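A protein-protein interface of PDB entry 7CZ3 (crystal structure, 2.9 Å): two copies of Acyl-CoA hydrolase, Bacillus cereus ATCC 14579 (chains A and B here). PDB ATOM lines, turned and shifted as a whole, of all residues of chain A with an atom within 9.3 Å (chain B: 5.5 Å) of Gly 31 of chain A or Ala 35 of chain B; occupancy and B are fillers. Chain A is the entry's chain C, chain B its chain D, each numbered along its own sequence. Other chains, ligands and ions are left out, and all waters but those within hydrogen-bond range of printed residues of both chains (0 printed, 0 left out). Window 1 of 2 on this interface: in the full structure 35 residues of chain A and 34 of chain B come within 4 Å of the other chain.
Of the printed residues of chain B, Gly 30 of chain A touches Asp 38 (3.5 Å).
Of chain B, only Ala 35 (3.9 Å) and Asp 38 (3.1 Å) come within 4 Å of Gly 31 of chain A.
Tyr 75 of chain A touches none of the printed residues of chain B.
Of the printed residues of chain A, Gly 31 of chain B touches Ala 35 (3.8 Å) and Asp 38 (2.7 Å).
Lys 32 of chain B touches none of the printed residues of chain A.
Ala 35 of chain B touches just one residue of chain A: Gly 31 (3.9 Å).
The nearest residue of chain B that does not touch Gly 31 of chain A is Leu 34 of chain B (4.5 Å).
The nearest printed residue of chain B that does not touch Gly 30 of chain A is Leu 34 of chain B (6.3 Å).
N of Gly 31 of chain B sits at hydrogen-bond distance from OD2 of Asp 38 of chain A (2.7 Å).
OD2 of Asp 38 of chain A lies within hydrogen-bond range of N of Gly 30 of chain B (3.4 Å).
The backbone NH of Gly 31 of chain A sits at hydrogen-bond distance from the side-chain carboxylate of Asp 38 of chain B, 3.1 Å away.
Among the printed residues, merely in contact across the chains: Gly 30 of chain A with Asp 38 of chain B, Ala 35 of chain A with Gly 31 of chain B and Gly 31 of chain A with Ala 35 of chain B.
Gly 30 of chain A touches Asp 38 of chain B, and with the chains exchanged Asp 38 of chain A touches Gly 30 of chain B.
Gly 31 of chain A touches Ala 35 of chain B, and with the chains exchanged Ala 35 of chain A touches Gly 31 of chain B.
Gly 31 of chain A touches Asp 38 of chain B, and with the chains exchanged Asp 38 of chain A touches Gly 31 of chain B.
Of the 6 pairs that touch across the chains among the printed residues, 6 have their exchanged pair printed and touching as well.
Of the 18 printed residues of chain A, 4 touch a printed residue of chain B.
Printed residues of chain A that touch a printed residue of chain B: Gly 30, Gly 31, Ala 35 and Asp 38.
Of the 11 printed residues of chain B, 4 touch a printed residue of chain A.
Along chain B the printed residues that touch a printed residue of chain A span positions 30 to 38.
Among the printed residues, no Asp or Glu carboxylate lies within 4 Å of a Lys or Arg side-chain nitrogen of the other chain.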
ATOM      1  N   ASP A  21      -6.870   4.054 -34.842  1.00  0.00           N
ATOM      2  CA  ASP A  21      -5.710   3.437 -34.136  1.00  0.00           C
ATOM      3  C   ASP A  21      -4.388   3.935 -34.732  1.00  0.00           C
ATOM      4  O   ASP A  21      -3.322   3.409 -34.292  1.00  0.00           O
ATOM      5  CB  ASP A  21      -5.748   1.914 -34.220  1.00  0.00           C
ATOM      6  CG  ASP A  21      -6.906   1.281 -33.487  1.00  0.00           C
ATOM      7  OD1 ASP A  21      -7.250   1.807 -32.392  1.00  0.00           O
ATOM      8  OD2 ASP A  21      -7.436   0.267 -34.011  1.00  0.00           O
ATOM      9  N   THR A  27       0.463   6.490 -38.348  1.00  0.00           N
ATOM     10  CA  THR A  27       1.065   5.142 -38.234  1.00  0.00           C
ATOM     11  C   THR A  27       0.409   4.451 -37.040  1.00  0.00           C
ATOM     12  O   THR A  27      -0.024   5.140 -36.134  1.00  0.00           O
ATOM     13  CB  THR A  27       2.582   5.221 -38.070  1.00  0.00           C
ATOM     14  OG1 THR A  27       2.794   6.008 -36.908  1.00  0.00           O
ATOM     15  CG2 THR A  27       3.266   5.888 -39.237  1.00  0.00           C
ATOM     16  N   LEU A  28       0.381   3.130 -37.036  1.00  0.00           N
ATOM     17  CA  LEU A  28      -0.321   2.392 -35.965  1.00  0.00           C
ATOM     18  C   LEU A  28       0.329   2.579 -34.593  1.00  0.00           C
ATOM     19  O   LEU A  28       1.538   2.500 -34.513  1.00  0.00           O
ATOM     20  CB  LEU A  28      -0.312   0.917 -36.359  1.00  0.00           C
ATOM     21  CG  LEU A  28      -1.067  -0.014 -35.425  1.00  0.00           C
ATOM     22  CD1 LEU A  28      -2.491   0.460 -35.257  1.00  0.00           C
ATOM     23  CD2 LEU A  28      -1.055  -1.424 -35.958  1.00  0.00           C
ATOM     24  N   PHE A  29      -0.481   2.875 -33.577  1.00  0.00           N
ATOM     25  CA  PHE A  29      -0.060   2.875 -32.145  1.00  0.00           C
ATOM     26  C   PHE A  29       0.473   1.506 -31.695  1.00  0.00           C
ATOM     27  O   PHE A  29      -0.086   0.467 -32.093  1.00  0.00           O
ATOM     28  CB  PHE A  29      -1.230   3.097 -31.185  1.00  0.00           C
ATOM     29  CG  PHE A  29      -1.881   4.447 -31.227  1.00  0.00           C
ATOM     30  CD1 PHE A  29      -1.134   5.593 -31.038  1.00  0.00           C
ATOM     31  CD2 PHE A  29      -3.253   4.559 -31.386  1.00  0.00           C
ATOM     32  CE1 PHE A  29      -1.745   6.835 -31.077  1.00  0.00           C
ATOM     33  CE2 PHE A  29      -3.860   5.802 -31.425  1.00  0.00           C
ATOM     34  CZ  PHE A  29      -3.105   6.937 -31.268  1.00  0.00           C
ATOM     35  N   GLY A  30       1.441   1.514 -30.775  1.00  0.00           N
ATOM     36  CA  GLY A  30       1.998   0.301 -30.147  1.00  0.00           C
ATOM     37  C   GLY A  30       0.923  -0.452 -29.405  1.00  0.00           C
ATOM     38  O   GLY A  30       0.768  -1.682 -29.653  1.00  0.00           O
ATOM     39  N   GLY A  31       0.158   0.284 -28.581  1.00  0.00           N
ATOM     40  CA  GLY A  31      -0.913  -0.259 -27.722  1.00  0.00           C
ATOM     41  C   GLY A  31      -1.853  -1.162 -28.506  1.00  0.00           C
ATOM     42  O   GLY A  31      -2.209  -2.264 -27.992  1.00  0.00           O
ATOM     43  N   LYS A  32      -2.238  -0.739 -29.717  1.00  0.00           N
ATOM     44  CA  LYS A  32      -3.204  -1.517 -30.533  1.00  0.00           C
ATOM     45  C   LYS A  32      -2.543  -2.881 -30.741  1.00  0.00           C
ATOM     46  O   LYS A  32      -3.161  -3.930 -30.386  1.00  0.00           O
ATOM     47  CB  LYS A  32      -3.560  -0.760 -31.823  1.00  0.00           C
ATOM     48  CG  LYS A  32      -4.481  -1.485 -32.793  1.00  0.00           C
ATOM     49  CD  LYS A  32      -5.762  -1.860 -32.171  1.00  0.00           C
ATOM     50  CE  LYS A  32      -6.654  -2.646 -33.099  1.00  0.00           C
ATOM     51  NZ  LYS A  32      -7.827  -3.131 -32.337  1.00  0.00           N
ATOM     52  N   LEU A  33      -1.280  -2.843 -31.175  1.00  0.00           N
ATOM     53  CA  LEU A  33      -0.512  -4.073 -31.478  1.00  0.00           C
ATOM     54  C   LEU A  33      -0.434  -4.979 -30.248  1.00  0.00           C
ATOM     55  O   LEU A  33      -0.638  -6.209 -30.385  1.00  0.00           O
ATOM     56  CB  LEU A  33       0.888  -3.692 -31.946  1.00  0.00           C
ATOM     57  CG  LEU A  33       1.554  -4.769 -32.783  1.00  0.00           C
ATOM     58  CD1 LEU A  33       0.839  -4.880 -34.120  1.00  0.00           C
ATOM     59  CD2 LEU A  33       3.018  -4.445 -32.978  1.00  0.00           C
ATOM     60  N   LEU A  34      -0.131  -4.410 -29.084  1.00  0.00           N
ATOM     61  CA  LEU A  34       0.031  -5.241 -27.864  1.00  0.00           C
ATOM     62  C   LEU A  34      -1.326  -5.866 -27.533  1.00  0.00           C
ATOM     63  O   LEU A  34      -1.330  -7.077 -27.189  1.00  0.00           O
ATOM     64  CB  LEU A  34       0.603  -4.400 -26.720  1.00  0.00           C
ATOM     65  CG  LEU A  34       2.076  -4.013 -26.868  1.00  0.00           C
ATOM     66  CD1 LEU A  34       2.471  -2.937 -25.863  1.00  0.00           C
ATOM     67  CD2 LEU A  34       2.975  -5.234 -26.721  1.00  0.00           C
ATOM     68  N   ALA A  35      -2.421  -5.108 -27.741  1.00  0.00           N
ATOM     69  CA  ALA A  35      -3.814  -5.519 -27.448  1.00  0.00           C
ATOM     70  C   ALA A  35      -4.183  -6.698 -28.338  1.00  0.00           C
ATOM     71  O   ALA A  35      -4.748  -7.712 -27.848  1.00  0.00           O
ATOM     72  CB  ALA A  35      -4.756  -4.370 -27.664  1.00  0.00           C
ATOM     73  N   GLU A  36      -3.843  -6.575 -29.613  1.00  0.00           N
ATOM     74  CA  GLU A  36      -4.087  -7.649 -30.603  1.00  0.00           C
ATOM     75  C   GLU A  36      -3.274  -8.906 -30.237  1.00  0.00           C
ATOM     76  O   GLU A  36      -3.842 -10.034 -30.343  1.00  0.00           O
ATOM     77  CB  GLU A  36      -3.750  -7.126 -31.994  1.00  0.00           C
ATOM     78  CG  GLU A  36      -4.662  -7.708 -33.049  1.00  0.00           C
ATOM     79  CD  GLU A  36      -6.084  -7.187 -32.991  1.00  0.00           C
ATOM     80  OE1 GLU A  36      -6.283  -6.065 -33.465  1.00  0.00           O
ATOM     81  OE2 GLU A  36      -6.972  -7.913 -32.480  1.00  0.00           O
ATOM     82  N   ILE A  37      -2.009  -8.727 -29.820  1.00  0.00           N
ATOM     83  CA  ILE A  37      -1.094  -9.835 -29.418  1.00  0.00           C
ATOM     84  C   ILE A  37      -1.681 -10.589 -28.220  1.00  0.00           C
ATOM     85  O   ILE A  37      -1.609 -11.822 -28.259  1.00  0.00           O
ATOM     86  CB  ILE A  37       0.302  -9.300 -29.083  1.00  0.00           C
ATOM     87  CG1 ILE A  37       1.034  -8.765 -30.314  1.00  0.00           C
ATOM     88  CG2 ILE A  37       1.104 -10.376 -28.385  1.00  0.00           C
ATOM     89  CD1 ILE A  37       2.234  -7.915 -29.982  1.00  0.00           C
ATOM     90  N   ASP A  38      -2.189  -9.878 -27.190  1.00  0.00           N
ATOM     91  CA  ASP A  38      -2.844 -10.485 -25.995  1.00  0.00           C
ATOM     92  C   ASP A  38      -4.077 -11.263 -26.481  1.00  0.00           C
ATOM     93  O   ASP A  38      -4.395 -12.377 -25.946  1.00  0.00           O
ATOM     94  CB  ASP A  38      -3.213  -9.419 -24.945  1.00  0.00           C
ATOM     95  CG  ASP A  38      -4.039  -9.888 -23.731  1.00  0.00           C
ATOM     96  OD1 ASP A  38      -3.573 -10.755 -22.973  1.00  0.00           O
ATOM     97  OD2 ASP A  38      -5.150  -9.355 -23.516  1.00  0.00           O
ATOM     98  N   SER A  39      -4.770 -10.698 -27.467  1.00  0.00           N
ATOM     99  CA  SER A  39      -6.074 -11.226 -27.921  1.00  0.00           C
ATOM    100  C   SER A  39      -5.831 -12.609 -28.519  1.00  0.00           C
ATOM    101  O   SER A  39      -6.386 -13.584 -28.005  1.00  0.00           O
ATOM    102  CB  SER A  39      -6.750 -10.263 -28.875  1.00  0.00           C
ATOM    103  OG  SER A  39      -8.165 -10.370 -28.805  1.00  0.00           O
ATOM    104  N   ILE A  58       4.155 -10.668 -19.900  1.00  0.00           N
ATOM    105  CA  ILE A  58       4.484 -10.490 -21.345  1.00  0.00           C
ATOM    106  C   ILE A  58       5.946 -10.039 -21.439  1.00  0.00           C
ATOM    107  O   ILE A  58       6.297  -9.015 -20.831  1.00  0.00           O
ATOM    108  CB  ILE A  58       3.523  -9.511 -22.071  1.00  0.00           C
ATOM    109  CG1 ILE A  58       3.741  -9.505 -23.587  1.00  0.00           C
ATOM    110  CG2 ILE A  58       3.623  -8.104 -21.512  1.00  0.00           C
ATOM    111  CD1 ILE A  58       3.122  -8.334 -24.301  1.00  0.00           C
ATOM    112  N   VAL A  61       8.719  -6.263 -25.786  1.00  0.00           N
ATOM    113  CA  VAL A  61       8.427  -6.263 -27.235  1.00  0.00           C
ATOM    114  C   VAL A  61       9.153  -5.069 -27.851  1.00  0.00           C
ATOM    115  O   VAL A  61       9.102  -3.967 -27.287  1.00  0.00           O
ATOM    116  CB  VAL A  61       6.920  -6.241 -27.519  1.00  0.00           C
ATOM    117  CG1 VAL A  61       6.680  -6.040 -28.996  1.00  0.00           C
ATOM    118  CG2 VAL A  61       6.225  -7.513 -27.046  1.00  0.00           C
ATOM    119  N   PHE A  63       9.404  -2.899 -31.296  1.00  0.00           N
ATOM    120  CA  PHE A  63       8.556  -2.484 -32.437  1.00  0.00           C
ATOM    121  C   PHE A  63       9.512  -2.217 -33.597  1.00  0.00           C
ATOM    122  O   PHE A  63      10.066  -1.118 -33.639  1.00  0.00           O
ATOM    123  CB  PHE A  63       7.628  -1.324 -32.028  1.00  0.00           C
ATOM    124  CG  PHE A  63       6.606  -1.700 -30.975  1.00  0.00           C
ATOM    125  CD1 PHE A  63       5.610  -2.628 -31.237  1.00  0.00           C
ATOM    126  CD2 PHE A  63       6.673  -1.185 -29.697  1.00  0.00           C
ATOM    127  CE1 PHE A  63       4.706  -3.018 -30.260  1.00  0.00           C
ATOM    128  CE2 PHE A  63       5.771  -1.580 -28.719  1.00  0.00           C
ATOM    129  CZ  PHE A  63       4.795  -2.502 -28.999  1.00  0.00           C
ATOM    130  N   TYR A  75      -1.406 -11.776 -37.194  1.00  0.00           N
ATOM    131  CA  TYR A  75      -0.978 -12.261 -35.868  1.00  0.00           C
ATOM    132  C   TYR A  75      -1.036 -13.790 -35.968  1.00  0.00           C
ATOM    133  O   TYR A  75      -2.097 -14.340 -36.278  1.00  0.00           O
ATOM    134  CB  TYR A  75      -1.802 -11.619 -34.733  1.00  0.00           C
ATOM    135  CG  TYR A  75      -1.850 -10.108 -34.696  1.00  0.00           C
ATOM    136  CD1 TYR A  75      -2.756  -9.416 -35.480  1.00  0.00           C
ATOM    137  CD2 TYR A  75      -1.069  -9.358 -33.830  1.00  0.00           C
ATOM    138  CE1 TYR A  75      -2.837  -8.036 -35.471  1.00  0.00           C
ATOM    139  CE2 TYR A  75      -1.127  -7.967 -33.811  1.00  0.00           C
ATOM    140  CZ  TYR A  75      -2.017  -7.303 -34.641  1.00  0.00           C
ATOM    141  OH  TYR A  75      -2.171  -5.945 -34.685  1.00  0.00           O
ATOM    142  N   GLY B  30      -5.168  -8.497 -20.259  1.00  0.00           N
ATOM    143  CA  GLY B  30      -3.836  -7.869 -20.170  1.00  0.00           C
ATOM    144  C   GLY B  30      -3.687  -6.803 -21.237  1.00  0.00           C
ATOM    145  O   GLY B  30      -2.912  -5.798 -21.029  1.00  0.00           O
ATOM    146  N   GLY B  31      -4.410  -6.995 -22.343  1.00  0.00           N
ATOM    147  CA  GLY B  31      -4.204  -6.184 -23.541  1.00  0.00           C
ATOM    148  C   GLY B  31      -4.773  -4.800 -23.335  1.00  0.00           C
ATOM    149  O   GLY B  31      -4.207  -3.830 -23.906  1.00  0.00           O
ATOM    150  N   LYS B  32      -5.880  -4.690 -22.589  1.00  0.00           N
ATOM    151  CA  LYS B  32      -6.540  -3.369 -22.426  1.00  0.00           C
ATOM    152  C   LYS B  32      -5.626  -2.554 -21.524  1.00  0.00           C
ATOM    153  O   LYS B  32      -5.403  -1.351 -21.820  1.00  0.00           O
ATOM    154  CB  LYS B  32      -7.962  -3.500 -21.879  1.00  0.00           C
ATOM    155  CG  LYS B  32      -8.683  -2.180 -21.624  1.00  0.00           C
ATOM    156  CD  LYS B  32      -8.884  -1.361 -22.878  1.00  0.00           C
ATOM    157  CE  LYS B  32      -9.689  -0.101 -22.648  1.00  0.00           C
ATOM    158  NZ  LYS B  32      -9.015   1.049 -23.288  1.00  0.00           N
ATOM    159  N   LEU B  33      -5.085  -3.229 -20.504  1.00  0.00           N
ATOM    160  CA  LEU B  33      -4.042  -2.684 -19.595  1.00  0.00           C
ATOM    161  C   LEU B  33      -2.852  -2.249 -20.460  1.00  0.00           C
ATOM    162  O   LEU B  33      -2.412  -1.051 -20.387  1.00  0.00           O
ATOM    163  CB  LEU B  33      -3.670  -3.743 -18.546  1.00  0.00           C
ATOM    164  CG  LEU B  33      -3.322  -3.193 -17.166  1.00  0.00           C
ATOM    165  CD1 LEU B  33      -4.538  -2.596 -16.500  1.00  0.00           C
ATOM    166  CD2 LEU B  33      -2.769  -4.262 -16.267  1.00  0.00           C
ATOM    167  N   LEU B  34      -2.375  -3.146 -21.314  1.00  0.00           N
ATOM    168  CA  LEU B  34      -1.137  -2.848 -22.075  1.00  0.00           C
ATOM    169  C   LEU B  34      -1.383  -1.678 -23.030  1.00  0.00           C
ATOM    170  O   LEU B  34      -0.431  -0.898 -23.243  1.00  0.00           O
ATOM    171  CB  LEU B  34      -0.668  -4.125 -22.761  1.00  0.00           C
ATOM    172  CG  LEU B  34      -0.085  -5.135 -21.775  1.00  0.00           C
ATOM    173  CD1 LEU B  34       0.001  -6.524 -22.392  1.00  0.00           C
ATOM    174  CD2 LEU B  34       1.282  -4.669 -21.292  1.00  0.00           C
ATOM    175  N   ALA B  35      -2.634  -1.530 -23.507  1.00  0.00           N
ATOM    176  CA  ALA B  35      -3.082  -0.514 -24.499  1.00  0.00           C
ATOM    177  C   ALA B  35      -3.149   0.831 -23.809  1.00  0.00           C
ATOM    178  O   ALA B  35      -2.704   1.847 -24.388  1.00  0.00           O
ATOM    179  CB  ALA B  35      -4.429  -0.858 -25.051  1.00  0.00           C
ATOM    180  N   GLU B  36      -3.682   0.784 -22.591  1.00  0.00           N
ATOM    181  CA  GLU B  36      -3.863   1.966 -21.728  1.00  0.00           C
ATOM    182  C   GLU B  36      -2.460   2.506 -21.393  1.00  0.00           C
ATOM    183  O   GLU B  36      -2.207   3.732 -21.664  1.00  0.00           O
ATOM    184  CB  GLU B  36      -4.746   1.553 -20.548  1.00  0.00           C
ATOM    185  CG  GLU B  36      -5.699   2.648 -20.101  1.00  0.00           C
ATOM    186  CD  GLU B  36      -6.978   2.886 -20.892  1.00  0.00           C
ATOM    187  OE1 GLU B  36      -7.919   2.048 -20.790  1.00  0.00           O
ATOM    188  OE2 GLU B  36      -7.058   3.942 -21.540  1.00  0.00           O
ATOM    189  N   ILE B  37      -1.570   1.627 -20.897  1.00  0.00           N
ATOM    190  CA  ILE B  37      -0.163   1.983 -20.571  1.00  0.00           C
ATOM    191  C   ILE B  37       0.426   2.716 -21.783  1.00  0.00           C
ATOM    192  O   ILE B  37       0.950   3.839 -21.615  1.00  0.00           O
ATOM    193  CB  ILE B  37       0.652   0.733 -20.189  1.00  0.00           C
ATOM    194  CG1 ILE B  37       0.332   0.259 -18.765  1.00  0.00           C
ATOM    195  CG2 ILE B  37       2.146   0.981 -20.397  1.00  0.00           C
ATOM    196  CD1 ILE B  37       0.633  -1.198 -18.486  1.00  0.00           C
ATOM    197  N   ASP B  38       0.335   2.147 -22.985  1.00  0.00           N
ATOM    198  CA  ASP B  38       1.002   2.821 -24.125  1.00  0.00           C
ATOM    199  C   ASP B  38       0.367   4.205 -24.331  1.00  0.00           C
ATOM    200  O   ASP B  38       1.078   5.160 -24.640  1.00  0.00           O
ATOM    201  CB  ASP B  38       0.967   1.991 -25.404  1.00  0.00           C
ATOM    202  CG  ASP B  38       1.737   2.681 -26.523  1.00  0.00           C
ATOM    203  OD1 ASP B  38       2.949   2.934 -26.303  1.00  0.00           O
ATOM    204  OD2 ASP B  38       1.112   3.014 -27.582  1.00  0.00           O
ATOM    205  N   SER B  39      -0.944   4.306 -24.156  1.00  0.00           N
ATOM    206  CA  SER B  39      -1.706   5.560 -24.386  1.00  0.00           C
ATOM    207  C   SER B  39      -1.280   6.650 -23.396  1.00  0.00           C
ATOM    208  O   SER B  39      -0.958   7.781 -23.840  1.00  0.00           O
ATOM    209  CB  SER B  39      -3.182   5.317 -24.306  1.00  0.00           C
ATOM    210  OG  SER B  39      -3.856   6.242 -25.144  1.00  0.00           O
ATOM    211  N   ILE B  40      -1.307   6.351 -22.100  1.00  0.00           N
ATOM    212  CA  ILE B  40      -1.018   7.383 -21.066  1.00  0.00           C
ATOM    213  C   ILE B  40       0.437   7.814 -21.255  1.00  0.00           C
ATOM    214  O   ILE B  40       0.680   9.038 -21.255  1.00  0.00           O
ATOM    215  CB  ILE B  40      -1.364   6.887 -19.641  1.00  0.00           C
ATOM    216  CG1 ILE B  40      -1.250   8.005 -18.599  1.00  0.00           C
ATOM    217  CG2 ILE B  40      -0.550   5.666 -19.234  1.00  0.00           C
ATOM    218  CD1 ILE B  40      -2.028   9.257 -18.945  1.00  0.00           C
